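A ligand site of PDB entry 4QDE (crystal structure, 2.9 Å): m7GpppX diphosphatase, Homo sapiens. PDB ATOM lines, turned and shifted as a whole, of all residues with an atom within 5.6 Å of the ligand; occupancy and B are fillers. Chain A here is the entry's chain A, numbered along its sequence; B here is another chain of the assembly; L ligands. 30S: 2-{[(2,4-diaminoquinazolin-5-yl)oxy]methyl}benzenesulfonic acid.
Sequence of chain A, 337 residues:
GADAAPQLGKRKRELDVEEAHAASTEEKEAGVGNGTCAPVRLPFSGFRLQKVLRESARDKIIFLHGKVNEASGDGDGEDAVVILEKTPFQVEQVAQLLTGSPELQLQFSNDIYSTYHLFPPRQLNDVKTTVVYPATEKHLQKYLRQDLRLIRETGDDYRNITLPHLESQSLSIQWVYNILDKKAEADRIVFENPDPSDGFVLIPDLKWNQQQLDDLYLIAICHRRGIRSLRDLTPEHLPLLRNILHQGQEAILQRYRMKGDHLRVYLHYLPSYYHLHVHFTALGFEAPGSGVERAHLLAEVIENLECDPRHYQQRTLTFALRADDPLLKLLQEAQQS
The side-chain hydroxyl of Tyr 113 of chain B is bonded to a sulfur (S1) of the ligand (1.7 Å).
The side-chain carboxylate of Asp 205 lies within hydrogen-bond range of a nitrogen (N4) of the ligand, at 2.9 Å.
The side-chain carboxylate (OE2) of Glu 185 is in hydrogen-bond range of a nitrogen (N2) of the ligand (2.7 Å).
N3 of the ligand lies within hydrogen-bond range of O of Pro 204, 2.9 Å away.
O3 of the ligand sits close to OH of Tyr 273, at 3.0 Å.
The backbone NH (N) of Leu 206 is in hydrogen-bond range of a nitrogen (N1) of the ligand (3.1 Å).
NE1 of Trp 175 lies within hydrogen-bond range of O3 of the ligand (3.5 Å).
The backbone carbonyl oxygen (O) of Ile 203 lies within hydrogen-bond range of the backbone NH (N) of Ile 219 (2.9 Å).
The backbone carbonyl oxygen (O) of Pro 204 lies within hydrogen-bond range of the guanidinium group (NH2) of Arg 188 (2.8 Å).
NE2 of His 139 is in hydrogen-bond range of OH of Tyr 113 of chain B, 2.8 Å away.
NE of Arg 188 is in salt-bridge range of OE1 of Glu 185 (2.8 Å).
The side-chain hydroxyl of Tyr 143 sits close to a ring nitrogen (NE2) of His 139.
O of Trp 175 lies within hydrogen-bond range of ND2 of Asn 110 of chain B (3.0 Å).
The side-chain carboxylate (OE2) of Glu 185 sits at hydrogen-bond distance from the side-chain amide nitrogen (ND2) of Asn 110 of chain B (3.1 Å).
The side-chain amino group of Lys 207 lies within salt-bridge range of the side-chain carboxylate of Asp 205, 3.9 Å away.
His 139 touches the ligand (NE2 to O2, 3.7 Å).
Lys 142 touches the ligand.
OH of Tyr 143 touches C3 of the ligand (3.2 Å).
Ile 179 touches the ligand (CD1 to N2, 3.7 Å).
CG1 of Ile 203 touches N3 of the ligand (3.9 Å).
Ile 219 touches the ligand (CD1 to N1, 3.98 Å).
Asn 110 of chain B touches the ligand.
Hydrophobic or aromatic side chains within 4 Å of the ligand: Trp 175, Ile 179, Ile 203, Leu 206, Ile 219, Tyr 273 and Tyr 113 of chain B.
Within 4 Å of the ligand: His 139, Lys 142, Tyr 143, Trp 175, Ile 179, Glu 185, Ile 203, Pro 204, Asp 205, Leu 206, Ile 219, Tyr 273, Asn 110 of chain B and Tyr 113 of chain B.
Along chain A the residues within 4 Å of the ligand span positions 139 to 273.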
ATOM      1  N   ILE A  83      -9.704 -32.579  10.109  1.00  0.00           N
ATOM      2  CA  ILE A  83     -10.779 -31.705   9.593  1.00  0.00           C
ATOM      3  C   ILE A  83     -11.398 -32.389   8.353  1.00  0.00           C
ATOM      4  O   ILE A  83     -10.659 -32.766   7.447  1.00  0.00           O
ATOM      5  CB  ILE A  83     -10.308 -30.254   9.224  1.00  0.00           C
ATOM      6  CG1 ILE A  83      -9.150 -29.712  10.118  1.00  0.00           C
ATOM      7  CG2 ILE A  83     -11.501 -29.304   9.201  1.00  0.00           C
ATOM      8  CD1 ILE A  83      -9.286 -29.759  11.634  1.00  0.00           C
ATOM      9  N   THR A 130      -8.190 -32.667   6.071  1.00  0.00           N
ATOM     10  CA  THR A 130      -6.955 -32.034   6.506  1.00  0.00           C
ATOM     11  C   THR A 130      -6.512 -32.729   7.791  1.00  0.00           C
ATOM     12  O   THR A 130      -7.331 -32.925   8.681  1.00  0.00           O
ATOM     13  CB  THR A 130      -7.115 -30.505   6.600  1.00  0.00           C
ATOM     14  OG1 THR A 130      -7.585 -30.006   5.343  1.00  0.00           O
ATOM     15  CG2 THR A 130      -5.829 -29.794   6.965  1.00  0.00           C
ATOM     16  N   VAL A 132      -3.619 -32.801  10.944  1.00  0.00           N
ATOM     17  CA  VAL A 132      -2.608 -32.054  11.720  1.00  0.00           C
ATOM     18  C   VAL A 132      -1.911 -33.062  12.680  1.00  0.00           C
ATOM     19  O   VAL A 132      -2.451 -33.386  13.734  1.00  0.00           O
ATOM     20  CB  VAL A 132      -3.220 -30.837  12.480  1.00  0.00           C
ATOM     21  CG1 VAL A 132      -2.149 -30.011  13.169  1.00  0.00           C
ATOM     22  CG2 VAL A 132      -4.056 -29.954  11.559  1.00  0.00           C
ATOM     23  N   HIS A 139      -3.187 -25.890  19.555  1.00  0.00           N
ATOM     24  CA  HIS A 139      -3.739 -26.319  18.280  1.00  0.00           C
ATOM     25  C   HIS A 139      -5.186 -26.777  18.463  1.00  0.00           C
ATOM     26  O   HIS A 139      -6.021 -26.521  17.604  1.00  0.00           O
ATOM     27  CB  HIS A 139      -2.903 -27.433  17.645  1.00  0.00           C
ATOM     28  CG  HIS A 139      -2.522 -27.137  16.231  1.00  0.00           C
ATOM     29  ND1 HIS A 139      -1.227 -26.772  15.895  1.00  0.00           N
ATOM     30  CD2 HIS A 139      -3.293 -27.081  15.128  1.00  0.00           C
ATOM     31  CE1 HIS A 139      -1.249 -26.552  14.589  1.00  0.00           C
ATOM     32  NE2 HIS A 139      -2.475 -26.719  14.087  1.00  0.00           N
ATOM     33  N   LYS A 142      -7.666 -23.801  19.223  1.00  0.00           N
ATOM     34  CA  LYS A 142      -7.908 -23.100  17.974  1.00  0.00           C
ATOM     35  C   LYS A 142      -9.208 -23.478  17.287  1.00  0.00           C
ATOM     36  O   LYS A 142      -9.770 -22.632  16.591  1.00  0.00           O
ATOM     37  CB  LYS A 142      -6.734 -23.313  16.995  1.00  0.00           C
ATOM     38  CG  LYS A 142      -6.461 -22.105  16.125  1.00  0.00           C
ATOM     39  CD  LYS A 142      -5.823 -22.443  14.781  1.00  0.00           C
ATOM     40  CE  LYS A 142      -5.187 -21.225  14.168  1.00  0.00           C
ATOM     41  NZ  LYS A 142      -6.170 -20.134  13.905  1.00  0.00           N
ATOM     42  N   TYR A 143      -9.667 -24.730  17.433  1.00  0.00           N
ATOM     43  CA  TYR A 143     -10.889 -25.186  16.740  1.00  0.00           C
ATOM     44  C   TYR A 143     -12.100 -25.327  17.637  1.00  0.00           C
ATOM     45  O   TYR A 143     -13.135 -25.804  17.190  1.00  0.00           O
ATOM     46  CB  TYR A 143     -10.647 -26.489  15.956  1.00  0.00           C
ATOM     47  CG  TYR A 143      -9.342 -26.541  15.203  1.00  0.00           C
ATOM     48  CD1 TYR A 143      -9.120 -25.714  14.104  1.00  0.00           C
ATOM     49  CD2 TYR A 143      -8.335 -27.421  15.576  1.00  0.00           C
ATOM     50  CE1 TYR A 143      -7.896 -25.747  13.421  1.00  0.00           C
ATOM     51  CE2 TYR A 143      -7.130 -27.478  14.893  1.00  0.00           C
ATOM     52  CZ  TYR A 143      -6.910 -26.641  13.815  1.00  0.00           C
ATOM     53  OH  TYR A 143      -5.721 -26.720  13.145  1.00  0.00           O
ATOM     54  N   LEU A 171       2.107 -19.205  17.688  1.00  0.00           N
ATOM     55  CA  LEU A 171       2.295 -20.338  16.781  1.00  0.00           C
ATOM     56  C   LEU A 171       3.679 -20.416  16.061  1.00  0.00           C
ATOM     57  O   LEU A 171       4.358 -19.413  15.805  1.00  0.00           O
ATOM     58  CB  LEU A 171       1.171 -20.353  15.701  1.00  0.00           C
ATOM     59  CG  LEU A 171      -0.228 -20.888  16.069  1.00  0.00           C
ATOM     60  CD1 LEU A 171      -1.254 -20.530  15.001  1.00  0.00           C
ATOM     61  CD2 LEU A 171      -0.224 -22.403  16.291  1.00  0.00           C
ATOM     62  N   TRP A 175       5.403 -23.810   8.363  1.00  0.00           N
ATOM     63  CA  TRP A 175       4.728 -24.138   7.104  1.00  0.00           C
ATOM     64  C   TRP A 175       4.805 -22.968   6.118  1.00  0.00           C
ATOM     65  O   TRP A 175       4.904 -23.191   4.909  1.00  0.00           O
ATOM     66  CB  TRP A 175       3.269 -24.597   7.327  1.00  0.00           C
ATOM     67  CG  TRP A 175       2.346 -23.521   7.862  1.00  0.00           C
ATOM     68  CD1 TRP A 175       2.006 -23.306   9.162  1.00  0.00           C
ATOM     69  CD2 TRP A 175       1.611 -22.566   7.085  1.00  0.00           C
ATOM     70  NE1 TRP A 175       1.117 -22.259   9.251  1.00  0.00           N
ATOM     71  CE2 TRP A 175       0.845 -21.797   7.991  1.00  0.00           C
ATOM     72  CE3 TRP A 175       1.534 -22.266   5.707  1.00  0.00           C
ATOM     73  CZ2 TRP A 175       0.010 -20.746   7.568  1.00  0.00           C
ATOM     74  CZ3 TRP A 175       0.732 -21.220   5.291  1.00  0.00           C
ATOM     75  CH2 TRP A 175      -0.039 -20.482   6.215  1.00  0.00           C
ATOM     76  N   ILE A 179       6.990 -22.763   2.523  1.00  0.00           N
ATOM     77  CA  ILE A 179       6.451 -22.277   1.249  1.00  0.00           C
ATOM     78  C   ILE A 179       7.434 -21.294   0.624  1.00  0.00           C
ATOM     79  O   ILE A 179       7.819 -21.486  -0.520  1.00  0.00           O
ATOM     80  CB  ILE A 179       5.011 -21.709   1.368  1.00  0.00           C
ATOM     81  CG1 ILE A 179       3.992 -22.835   1.523  1.00  0.00           C
ATOM     82  CG2 ILE A 179       4.651 -20.824   0.179  1.00  0.00           C
ATOM     83  CD1 ILE A 179       2.748 -22.420   2.197  1.00  0.00           C
ATOM     84  N   GLU A 185       5.070 -27.160  -1.207  1.00  0.00           N
ATOM     85  CA  GLU A 185       4.050 -26.634  -2.121  1.00  0.00           C
ATOM     86  C   GLU A 185       4.600 -25.825  -3.310  1.00  0.00           C
ATOM     87  O   GLU A 185       3.870 -25.004  -3.873  1.00  0.00           O
ATOM     88  CB  GLU A 185       3.011 -25.794  -1.334  1.00  0.00           C
ATOM     89  CG  GLU A 185       2.057 -26.592  -0.460  1.00  0.00           C
ATOM     90  CD  GLU A 185       1.058 -25.736   0.294  1.00  0.00           C
ATOM     91  OE1 GLU A 185       0.055 -25.289  -0.325  1.00  0.00           O
ATOM     92  OE2 GLU A 185       1.266 -25.530   1.506  1.00  0.00           O
ATOM     93  N   ARG A 188       2.546 -25.627  -6.408  1.00  0.00           N
ATOM     94  CA  ARG A 188       1.270 -24.928  -6.230  1.00  0.00           C
ATOM     95  C   ARG A 188       1.386 -23.400  -6.382  1.00  0.00           C
ATOM     96  O   ARG A 188       0.350 -22.749  -6.474  1.00  0.00           O
ATOM     97  CB  ARG A 188       0.647 -25.277  -4.867  1.00  0.00           C
ATOM     98  CG  ARG A 188       0.373 -26.759  -4.642  1.00  0.00           C
ATOM     99  CD  ARG A 188      -0.316 -27.173  -3.345  1.00  0.00           C
ATOM    100  NE  ARG A 188      -1.176 -26.174  -2.674  1.00  0.00           N
ATOM    101  CZ  ARG A 188      -2.498 -26.140  -2.720  1.00  0.00           C
ATOM    102  NH1 ARG A 188      -3.177 -27.050  -3.408  1.00  0.00           N
ATOM    103  NH2 ARG A 188      -3.175 -25.230  -2.030  1.00  0.00           N
ATOM    104  N   ILE A 203      -0.154 -18.249  -3.596  1.00  0.00           N
ATOM    105  CA  ILE A 203      -0.441 -19.688  -3.561  1.00  0.00           C
ATOM    106  C   ILE A 203      -1.933 -19.946  -3.227  1.00  0.00           C
ATOM    107  O   ILE A 203      -2.489 -19.155  -2.465  1.00  0.00           O
ATOM    108  CB  ILE A 203       0.578 -20.344  -2.564  1.00  0.00           C
ATOM    109  CG1 ILE A 203       0.513 -21.899  -2.570  1.00  0.00           C
ATOM    110  CG2 ILE A 203       0.466 -19.770  -1.131  1.00  0.00           C
ATOM    111  CD1 ILE A 203       1.860 -22.606  -2.429  1.00  0.00           C
ATOM    112  N   PRO A 204      -2.609 -20.994  -3.796  1.00  0.00           N
ATOM    113  CA  PRO A 204      -3.990 -21.260  -3.387  1.00  0.00           C
ATOM    114  C   PRO A 204      -3.962 -21.707  -1.919  1.00  0.00           C
ATOM    115  O   PRO A 204      -3.101 -22.490  -1.509  1.00  0.00           O
ATOM    116  CB  PRO A 204      -4.434 -22.412  -4.314  1.00  0.00           C
ATOM    117  CG  PRO A 204      -3.397 -22.519  -5.353  1.00  0.00           C
ATOM    118  CD  PRO A 204      -2.139 -22.038  -4.730  1.00  0.00           C
ATOM    119  N   ASP A 205      -4.838 -21.123  -1.125  1.00  0.00           N
ATOM    120  CA  ASP A 205      -4.932 -21.400   0.295  1.00  0.00           C
ATOM    121  C   ASP A 205      -5.460 -22.795   0.484  1.00  0.00           C
ATOM    122  O   ASP A 205      -6.294 -23.248  -0.309  1.00  0.00           O
ATOM    123  CB  ASP A 205      -5.862 -20.382   0.961  1.00  0.00           C
ATOM    124  CG  ASP A 205      -5.957 -20.525   2.459  1.00  0.00           C
ATOM    125  OD1 ASP A 205      -6.766 -21.351   2.918  1.00  0.00           O
ATOM    126  OD2 ASP A 205      -5.155 -19.887   3.165  1.00  0.00           O
ATOM    127  N   LEU A 206      -4.986 -23.472   1.533  1.00  0.00           N
ATOM    128  CA  LEU A 206      -5.369 -24.813   1.995  1.00  0.00           C
ATOM    129  C   LEU A 206      -6.926 -25.009   2.063  1.00  0.00           C
ATOM    130  O   LEU A 206      -7.407 -26.135   1.846  1.00  0.00           O
ATOM    131  CB  LEU A 206      -4.732 -25.036   3.379  1.00  0.00           C
ATOM    132  CG  LEU A 206      -4.606 -26.461   3.863  1.00  0.00           C
ATOM    133  CD1 LEU A 206      -3.280 -26.668   4.536  1.00  0.00           C
ATOM    134  CD2 LEU A 206      -5.732 -26.819   4.807  1.00  0.00           C
ATOM    135  N   LYS A 207      -7.709 -23.927   2.379  1.00  0.00           N
ATOM    136  CA  LYS A 207      -9.189 -23.935   2.493  1.00  0.00           C
ATOM    137  C   LYS A 207      -9.888 -23.947   1.092  1.00  0.00           C
ATOM    138  O   LYS A 207     -11.124 -23.828   1.033  1.00  0.00           O
ATOM    139  CB  LYS A 207      -9.716 -22.769   3.403  1.00  0.00           C
ATOM    140  CG  LYS A 207      -9.127 -22.684   4.827  1.00  0.00           C
ATOM    141  CD  LYS A 207      -9.016 -21.206   5.376  1.00  0.00           C
ATOM    142  CE  LYS A 207      -7.682 -20.854   6.033  1.00  0.00           C
ATOM    143  NZ  LYS A 207      -7.489 -19.392   6.269  1.00  0.00           N
ATOM    144  N   ILE A 219      -3.789 -16.886  -1.301  1.00  0.00           N
ATOM    145  CA  ILE A 219      -3.079 -16.092  -0.291  1.00  0.00           C
ATOM    146  C   ILE A 219      -1.707 -15.649  -0.820  1.00  0.00           C
ATOM    147  O   ILE A 219      -0.984 -16.427  -1.451  1.00  0.00           O
ATOM    148  CB  ILE A 219      -3.006 -16.746   1.130  1.00  0.00           C
ATOM    149  CG1 ILE A 219      -2.254 -18.109   1.136  1.00  0.00           C
ATOM    150  CG2 ILE A 219      -4.377 -16.872   1.774  1.00  0.00           C
ATOM    151  CD1 ILE A 219      -1.568 -18.437   2.449  1.00  0.00           C
ATOM    152  N   TYR A 273      -1.621 -16.045  12.065  1.00  0.00           N
ATOM    153  CA  TYR A 273      -0.174 -16.247  11.894  1.00  0.00           C
ATOM    154  C   TYR A 273       0.448 -14.883  11.815  1.00  0.00           C
ATOM    155  O   TYR A 273       0.024 -14.036  11.026  1.00  0.00           O
ATOM    156  CB  TYR A 273       0.130 -17.127  10.631  1.00  0.00           C
ATOM    157  CG  TYR A 273      -0.872 -18.248  10.518  1.00  0.00           C
ATOM    158  CD1 TYR A 273      -0.945 -19.256  11.483  1.00  0.00           C
ATOM    159  CD2 TYR A 273      -1.894 -18.190   9.559  1.00  0.00           C
ATOM    160  CE1 TYR A 273      -2.000 -20.158  11.527  1.00  0.00           C
ATOM    161  CE2 TYR A 273      -2.939 -19.132   9.560  1.00  0.00           C
ATOM    162  CZ  TYR A 273      -2.988 -20.105  10.553  1.00  0.00           C
ATOM    163  OH  TYR A 273      -3.998 -21.050  10.574  1.00  0.00           O
ATOM    164  N   PHE B 108      -1.625 -32.351  -0.975  1.00  0.00           N
ATOM    165  CA  PHE B 108      -0.264 -31.873  -0.663  1.00  0.00           C
ATOM    166  C   PHE B 108       0.119 -32.086   0.806  1.00  0.00           C
ATOM    167  O   PHE B 108      -0.741 -32.278   1.684  1.00  0.00           O
ATOM    168  CB  PHE B 108      -0.007 -30.421  -1.109  1.00  0.00           C
ATOM    169  CG  PHE B 108      -0.844 -29.416  -0.378  1.00  0.00           C
ATOM    170  CD1 PHE B 108      -0.413 -28.867   0.824  1.00  0.00           C
ATOM    171  CD2 PHE B 108      -2.106 -29.049  -0.852  1.00  0.00           C
ATOM    172  CE1 PHE B 108      -1.213 -27.958   1.523  1.00  0.00           C
ATOM    173  CE2 PHE B 108      -2.897 -28.139  -0.148  1.00  0.00           C
ATOM    174  CZ  PHE B 108      -2.437 -27.586   1.024  1.00  0.00           C
ATOM    175  N   ASN B 110       2.772 -30.364   3.885  1.00  0.00           N
ATOM    176  CA  ASN B 110       3.567 -29.218   4.321  1.00  0.00           C
ATOM    177  C   ASN B 110       3.719 -29.276   5.852  1.00  0.00           C
ATOM    178  O   ASN B 110       2.769 -29.001   6.571  1.00  0.00           O
ATOM    179  CB  ASN B 110       2.982 -27.861   3.856  1.00  0.00           C
ATOM    180  CG  ASN B 110       3.775 -26.645   4.272  1.00  0.00           C
ATOM    181  OD1 ASN B 110       4.766 -26.716   4.968  1.00  0.00           O
ATOM    182  ND2 ASN B 110       3.370 -25.481   3.805  1.00  0.00           N
ATOM    183  N   TYR B 113       1.166 -30.421   8.682  1.00  0.00           N
ATOM    184  CA  TYR B 113      -0.059 -30.291   7.923  1.00  0.00           C
ATOM    185  C   TYR B 113      -0.026 -31.117   6.624  1.00  0.00           C
ATOM    186  O   TYR B 113       0.984 -31.147   5.922  1.00  0.00           O
ATOM    187  CB  TYR B 113      -0.278 -28.795   7.611  1.00  0.00           C
ATOM    188  CG  TYR B 113      -0.692 -27.926   8.785  1.00  0.00           C
ATOM    189  CD1 TYR B 113      -2.018 -27.858   9.191  1.00  0.00           C
ATOM    190  CD2 TYR B 113       0.221 -27.049   9.386  1.00  0.00           C
ATOM    191  CE1 TYR B 113      -2.418 -27.022  10.233  1.00  0.00           C
ATOM    192  CE2 TYR B 113      -0.179 -26.182  10.418  1.00  0.00           C
ATOM    193  CZ  TYR B 113      -1.518 -26.128  10.792  1.00  0.00           C
ATOM    194  OH  TYR B 113      -1.973 -25.252  11.793  1.00  0.00           O
HETATM  195  C1  30S L   1      -5.629 -25.201   8.266  1.00  0.00           C
HETATM  196  C2  30S L   1      -5.798 -25.483   9.596  1.00  0.00           C
HETATM  197  C3  30S L   1      -4.919 -24.977  10.534  1.00  0.00           C
HETATM  198  C4  30S L   1      -3.855 -24.197  10.116  1.00  0.00           C
HETATM  199  C5  30S L   1      -3.671 -23.863   8.763  1.00  0.00           C
HETATM  200  C6  30S L   1      -4.579 -24.393   7.842  1.00  0.00           C
HETATM  201  C7  30S L   1      -2.599 -22.921   8.280  1.00  0.00           C
HETATM  202  O1  30S L   1      -2.547 -22.865   6.843  1.00  0.00           O
HETATM  203  C8  30S L   1      -1.761 -23.756   6.161  1.00  0.00           C
HETATM  204  C9  30S L   1      -0.995 -24.753   6.721  1.00  0.00           C
HETATM  205  C10 30S L   1      -0.086 -25.453   5.949  1.00  0.00           C
HETATM  206  C11 30S L   1       0.047 -25.197   4.608  1.00  0.00           C
HETATM  207  C12 30S L   1      -0.739 -24.195   4.002  1.00  0.00           C
HETATM  208  C13 30S L   1      -1.684 -23.450   4.780  1.00  0.00           C
HETATM  209  C14 30S L   1      -2.462 -22.503   3.977  1.00  0.00           C
HETATM  210  N1  30S L   1      -2.320 -22.337   2.670  1.00  0.00           N
HETATM  211  C15 30S L   1      -1.384 -23.088   2.049  1.00  0.00           C
HETATM  212  N2  30S L   1      -0.577 -23.996   2.651  1.00  0.00           N
HETATM  213  N3  30S L   1      -1.261 -22.935   0.719  1.00  0.00           N
HETATM  214  N4  30S L   1      -3.421 -21.757   4.561  1.00  0.00           N
HETATM  215  S1  30S L   1      -2.790 -23.851  11.428  1.00  0.00           S
HETATM  216  O2  30S L   1      -3.544 -23.529  12.576  1.00  0.00           O
HETATM  217  O3  30S L   1      -1.768 -22.966  11.028  1.00  0.00           O
